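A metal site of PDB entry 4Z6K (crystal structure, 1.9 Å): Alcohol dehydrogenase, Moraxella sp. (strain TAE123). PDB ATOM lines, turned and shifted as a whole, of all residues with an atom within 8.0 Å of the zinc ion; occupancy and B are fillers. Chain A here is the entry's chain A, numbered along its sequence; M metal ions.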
ATOM      1  N   SER A  90       4.043  28.020  25.362  1.00  0.00           N
ATOM      2  CA  SER A  90       3.019  27.941  26.370  1.00  0.00           C
ATOM      3  C   SER A  90       2.390  26.565  26.292  1.00  0.00           C
ATOM      4  O   SER A  90       2.486  25.874  25.253  1.00  0.00           O
ATOM      5  CB  SER A  90       1.898  28.997  26.187  1.00  0.00           C
ATOM      6  OG  SER A  90       1.168  28.772  25.007  1.00  0.00           O
ATOM      7  N   ALA A  91       1.731  26.223  27.364  1.00  0.00           N
ATOM      8  CA  ALA A  91       0.909  24.970  27.465  1.00  0.00           C
ATOM      9  C   ALA A  91      -0.255  25.280  28.373  1.00  0.00           C
ATOM     10  O   ALA A  91      -0.271  26.342  28.962  1.00  0.00           O
ATOM     11  CB  ALA A  91       1.737  23.871  28.046  1.00  0.00           C
ATOM     12  N   CYS A  92      -1.199  24.365  28.563  1.00  0.00           N
ATOM     13  CA  CYS A  92      -2.512  24.858  29.009  1.00  0.00           C
ATOM     14  C   CYS A  92      -2.505  24.941  30.529  1.00  0.00           C
ATOM     15  O   CYS A  92      -3.229  25.693  31.145  1.00  0.00           O
ATOM     16  CB  CYS A  92      -3.636  23.951  28.494  1.00  0.00           C
ATOM     17  SG  CYS A  92      -3.655  22.257  29.196  1.00  0.00           S
ATOM     18  N   GLY A  93      -1.690  24.084  31.107  1.00  0.00           N
ATOM     19  CA  GLY A  93      -1.502  23.970  32.514  1.00  0.00           C
ATOM     20  C   GLY A  93      -2.552  23.188  33.269  1.00  0.00           C
ATOM     21  O   GLY A  93      -2.473  23.100  34.484  1.00  0.00           O
ATOM     22  N   HIS A  94      -3.535  22.615  32.552  1.00  0.00           N
ATOM     23  CA  HIS A  94      -4.686  21.988  33.179  1.00  0.00           C
ATOM     24  C   HIS A  94      -4.848  20.520  32.796  1.00  0.00           C
ATOM     25  O   HIS A  94      -5.535  19.821  33.465  1.00  0.00           O
ATOM     26  CB  HIS A  94      -6.030  22.718  32.827  1.00  0.00           C
ATOM     27  CG  HIS A  94      -5.916  24.190  32.700  1.00  0.00           C
ATOM     28  ND1 HIS A  94      -6.320  24.863  31.561  1.00  0.00           N
ATOM     29  CD2 HIS A  94      -5.445  25.149  33.558  1.00  0.00           C
ATOM     30  CE1 HIS A  94      -6.063  26.158  31.711  1.00  0.00           C
ATOM     31  NE2 HIS A  94      -5.559  26.360  32.917  1.00  0.00           N
ATOM     32  N   CYS A  95      -4.232  20.066  31.714  1.00  0.00           N
ATOM     33  CA  CYS A  95      -4.469  18.684  31.217  1.00  0.00           C
ATOM     34  C   CYS A  95      -3.614  17.702  31.985  1.00  0.00           C
ATOM     35  O   CYS A  95      -2.681  18.072  32.704  1.00  0.00           O
ATOM     36  CB  CYS A  95      -4.131  18.756  29.686  1.00  0.00           C
ATOM     37  SG  CYS A  95      -2.486  18.711  29.246  1.00  0.00           S
ATOM     38  N   THR A  96      -3.873  16.430  31.828  1.00  0.00           N
ATOM     39  CA  THR A  96      -3.014  15.412  32.406  1.00  0.00           C
ATOM     40  C   THR A  96      -1.532  15.528  32.131  1.00  0.00           C
ATOM     41  O   THR A  96      -0.716  15.371  33.038  1.00  0.00           O
ATOM     42  CB  THR A  96      -3.535  14.042  32.010  1.00  0.00           C
ATOM     43  OG1 THR A  96      -4.874  13.918  32.492  1.00  0.00           O
ATOM     44  CG2 THR A  96      -2.733  12.923  32.621  1.00  0.00           C
ATOM     45  N   HIS A  97      -1.141  15.851  30.890  1.00  0.00           N
ATOM     46  CA  HIS A  97       0.197  15.960  30.597  1.00  0.00           C
ATOM     47  C   HIS A  97       0.779  17.144  31.382  1.00  0.00           C
ATOM     48  O   HIS A  97       1.875  17.019  31.905  1.00  0.00           O
ATOM     49  CB  HIS A  97       0.366  16.271  29.085  1.00  0.00           C
ATOM     50  CG  HIS A  97      -0.101  15.178  28.176  1.00  0.00           C
ATOM     51  ND1 HIS A  97       0.301  13.865  28.319  1.00  0.00           N
ATOM     52  CD2 HIS A  97      -0.839  15.217  27.053  1.00  0.00           C
ATOM     53  CE1 HIS A  97      -0.179  13.141  27.327  1.00  0.00           C
ATOM     54  NE2 HIS A  97      -0.894  13.940  26.554  1.00  0.00           N
ATOM     55  N   CYS A  98       0.147  18.331  31.339  1.00  0.00           N
ATOM     56  CA  CYS A  98       0.654  19.497  32.051  1.00  0.00           C
ATOM     57  C   CYS A  98       0.672  19.231  33.571  1.00  0.00           C
ATOM     58  O   CYS A  98       1.672  19.560  34.208  1.00  0.00           O
ATOM     59  CB  CYS A  98      -0.226  20.770  31.782  1.00  0.00           C
ATOM     60  SG  CYS A  98      -0.004  21.315  30.103  1.00  0.00           S
ATOM     61  N   LEU A  99      -0.280  18.505  34.103  1.00  0.00           N
ATOM     62  CA  LEU A  99      -0.321  18.357  35.587  1.00  0.00           C
ATOM     63  C   LEU A  99       0.821  17.433  36.076  1.00  0.00           C
ATOM     64  O   LEU A  99       1.194  17.440  37.260  1.00  0.00           O
ATOM     65  CB  LEU A  99      -1.690  17.861  36.052  1.00  0.00           C
ATOM     66  CG  LEU A  99      -2.879  18.794  35.905  1.00  0.00           C
ATOM     67  CD1 LEU A  99      -4.171  18.185  36.467  1.00  0.00           C
ATOM     68  CD2 LEU A  99      -2.533  20.088  36.646  1.00  0.00           C
ATOM     69  N   TRP A 102       4.730  16.788  32.175  1.00  0.00           N
ATOM     70  CA  TRP A 102       4.962  16.405  30.797  1.00  0.00           C
ATOM     71  C   TRP A 102       4.280  17.383  29.904  1.00  0.00           C
ATOM     72  O   TRP A 102       3.656  17.051  28.897  1.00  0.00           O
ATOM     73  CB  TRP A 102       4.425  15.005  30.562  1.00  0.00           C
ATOM     74  CG  TRP A 102       5.376  13.924  30.995  1.00  0.00           C
ATOM     75  CD1 TRP A 102       5.277  13.156  32.094  1.00  0.00           C
ATOM     76  CD2 TRP A 102       6.532  13.434  30.269  1.00  0.00           C
ATOM     77  NE1 TRP A 102       6.283  12.241  32.118  1.00  0.00           N
ATOM     78  CE2 TRP A 102       7.075  12.405  31.019  1.00  0.00           C
ATOM     79  CE3 TRP A 102       7.121  13.786  29.069  1.00  0.00           C
ATOM     80  CZ2 TRP A 102       8.200  11.710  30.615  1.00  0.00           C
ATOM     81  CZ3 TRP A 102       8.268  13.082  28.638  1.00  0.00           C
ATOM     82  CH2 TRP A 102       8.793  12.106  29.415  1.00  0.00           C
ATOM     83  N   GLU A 103       4.575  18.677  30.120  1.00  0.00           N
ATOM     84  CA  GLU A 103       3.892  19.733  29.394  1.00  0.00           C
ATOM     85  C   GLU A 103       4.301  19.737  27.926  1.00  0.00           C
ATOM     86  O   GLU A 103       3.629  20.331  27.122  1.00  0.00           O
ATOM     87  CB  GLU A 103       4.081  21.123  30.050  1.00  0.00           C
ATOM     88  CG  GLU A 103       5.503  21.626  30.176  1.00  0.00           C
ATOM     89  CD  GLU A 103       6.150  21.365  31.521  1.00  0.00           C
ATOM     90  OE1 GLU A 103       5.791  20.329  32.203  1.00  0.00           O
ATOM     91  OE2 GLU A 103       7.044  22.167  31.882  1.00  0.00           O
ATOM     92  N   THR A 104       5.460  19.119  27.626  1.00  0.00           N
ATOM     93  CA  THR A 104       5.917  19.000  26.276  1.00  0.00           C
ATOM     94  C   THR A 104       4.906  18.221  25.417  1.00  0.00           C
ATOM     95  O   THR A 104       4.983  18.297  24.176  1.00  0.00           O
ATOM     96  CB  THR A 104       7.297  18.298  26.193  1.00  0.00           C
ATOM     97  OG1 THR A 104       7.287  17.110  27.023  1.00  0.00           O
ATOM     98  CG2 THR A 104       8.356  19.225  26.659  1.00  0.00           C
ATOM     99  N   LEU A 105       3.968  17.515  26.054  1.00  0.00           N
ATOM    100  CA  LEU A 105       3.034  16.679  25.337  1.00  0.00           C
ATOM    101  C   LEU A 105       1.698  17.379  25.208  1.00  0.00           C
ATOM    102  O   LEU A 105       0.780  16.855  24.556  1.00  0.00           O
ATOM    103  CB  LEU A 105       2.879  15.341  25.988  1.00  0.00           C
ATOM    104  CG  LEU A 105       4.138  14.452  26.093  1.00  0.00           C
ATOM    105  CD1 LEU A 105       3.764  13.105  26.679  1.00  0.00           C
ATOM    106  CD2 LEU A 105       4.787  14.288  24.732  1.00  0.00           C
ATOM    107  N   CYS A 106       1.606  18.608  25.711  1.00  0.00           N
ATOM    108  CA  CYS A 106       0.283  19.268  25.814  1.00  0.00           C
ATOM    109  C   CYS A 106      -0.300  19.501  24.399  1.00  0.00           C
ATOM    110  O   CYS A 106       0.394  19.993  23.523  1.00  0.00           O
ATOM    111  CB  CYS A 106       0.371  20.544  26.659  1.00  0.00           C
ATOM    112  SG  CYS A 106      -1.136  21.484  26.579  1.00  0.00           S
ATOM    113  N   GLU A 107      -1.524  19.019  24.192  1.00  0.00           N
ATOM    114  CA  GLU A 107      -2.140  19.058  22.895  1.00  0.00           C
ATOM    115  C   GLU A 107      -2.515  20.495  22.466  1.00  0.00           C
ATOM    116  O   GLU A 107      -2.843  20.691  21.343  1.00  0.00           O
ATOM    117  CB  GLU A 107      -3.378  18.175  22.821  1.00  0.00           C
ATOM    118  CG  GLU A 107      -3.203  16.673  23.082  1.00  0.00           C
ATOM    119  CD  GLU A 107      -2.672  15.860  21.902  1.00  0.00           C
ATOM    120  OE1 GLU A 107      -2.337  16.479  20.859  1.00  0.00           O
ATOM    121  OE2 GLU A 107      -2.597  14.617  21.993  1.00  0.00           O
ATOM    122  N   SER A 108      -2.517  21.471  23.363  1.00  0.00           N
ATOM    123  CA  SER A 108      -2.787  22.817  23.003  1.00  0.00           C
ATOM    124  C   SER A 108      -1.606  23.739  23.196  1.00  0.00           C
ATOM    125  O   SER A 108      -1.722  24.947  23.320  1.00  0.00           O
ATOM    126  CB  SER A 108      -4.030  23.360  23.667  1.00  0.00           C
ATOM    127  OG  SER A 108      -4.175  22.938  24.969  1.00  0.00           O
ATOM    128  N   GLN A 109      -0.426  23.156  23.149  1.00  0.00           N
ATOM    129  CA  GLN A 109       0.734  23.981  23.356  1.00  0.00           C
ATOM    130  C   GLN A 109       0.855  24.912  22.214  1.00  0.00           C
ATOM    131  O   GLN A 109       0.373  24.633  21.149  1.00  0.00           O
ATOM    132  CB  GLN A 109       2.044  23.178  23.465  1.00  0.00           C
ATOM    133  CG  GLN A 109       2.474  22.497  22.195  1.00  0.00           C
ATOM    134  CD  GLN A 109       3.595  21.512  22.447  1.00  0.00           C
ATOM    135  OE1 GLN A 109       4.763  21.819  22.164  1.00  0.00           O
ATOM    136  NE2 GLN A 109       3.275  20.369  23.021  1.00  0.00           N
ATOM    137  N   TYR A 130       6.687  30.299  30.890  1.00  0.00           N
ATOM    138  CA  TYR A 130       7.346  29.318  30.104  1.00  0.00           C
ATOM    139  C   TYR A 130       8.773  29.732  29.619  1.00  0.00           C
ATOM    140  O   TYR A 130       9.436  28.964  28.979  1.00  0.00           O
ATOM    141  CB  TYR A 130       6.416  28.921  28.937  1.00  0.00           C
ATOM    142  CG  TYR A 130       5.279  28.137  29.426  1.00  0.00           C
ATOM    143  CD1 TYR A 130       4.138  28.767  29.863  1.00  0.00           C
ATOM    144  CD2 TYR A 130       5.351  26.751  29.603  1.00  0.00           C
ATOM    145  CE1 TYR A 130       3.143  28.077  30.496  1.00  0.00           C
ATOM    146  CE2 TYR A 130       4.338  26.043  30.193  1.00  0.00           C
ATOM    147  CZ  TYR A 130       3.192  26.691  30.580  1.00  0.00           C
ATOM    148  OH  TYR A 130       2.131  26.021  31.195  1.00  0.00           O
HETATM  149 ZN    ZN M   1      -1.873  20.979  28.796  1.00  0.00          ZN
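A ring nitrogen (NE2) of His 94 lies close to the backbone carbonyl oxygen (O) of Cys 92 (3.0 Å). The backbone NH (N) of His 97 sits close to the side-chain sulfur (SG) of Cys 95 (3.6 Å). N of Gly 93 lies close to SG of Cys 98 (3.4 Å). The side-chain amide nitrogen (NE2) of Gln 109 is in hydrogen-bond range of the backbone carbonyl oxygen (O) of Cys 106 (2.9 Å). The backbone NH of Ser 108 lies close to the side-chain sulfur of Cys 106.
Merely in contact with the zinc ion: Gly 93 (3.9 Å).
The zinc ion is bound by SG of Cys 92, 2.2 Å away. The zinc ion is bound by the side-chain sulfur (SG) of Cys 98 (2.3 Å). The zinc ion is bound by SG of Cys 106. The zinc ion is bound by the side-chain sulfur (SG) of Cys 95, at 2.4 Å. The zinc ion has four donor atoms within binding distance.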
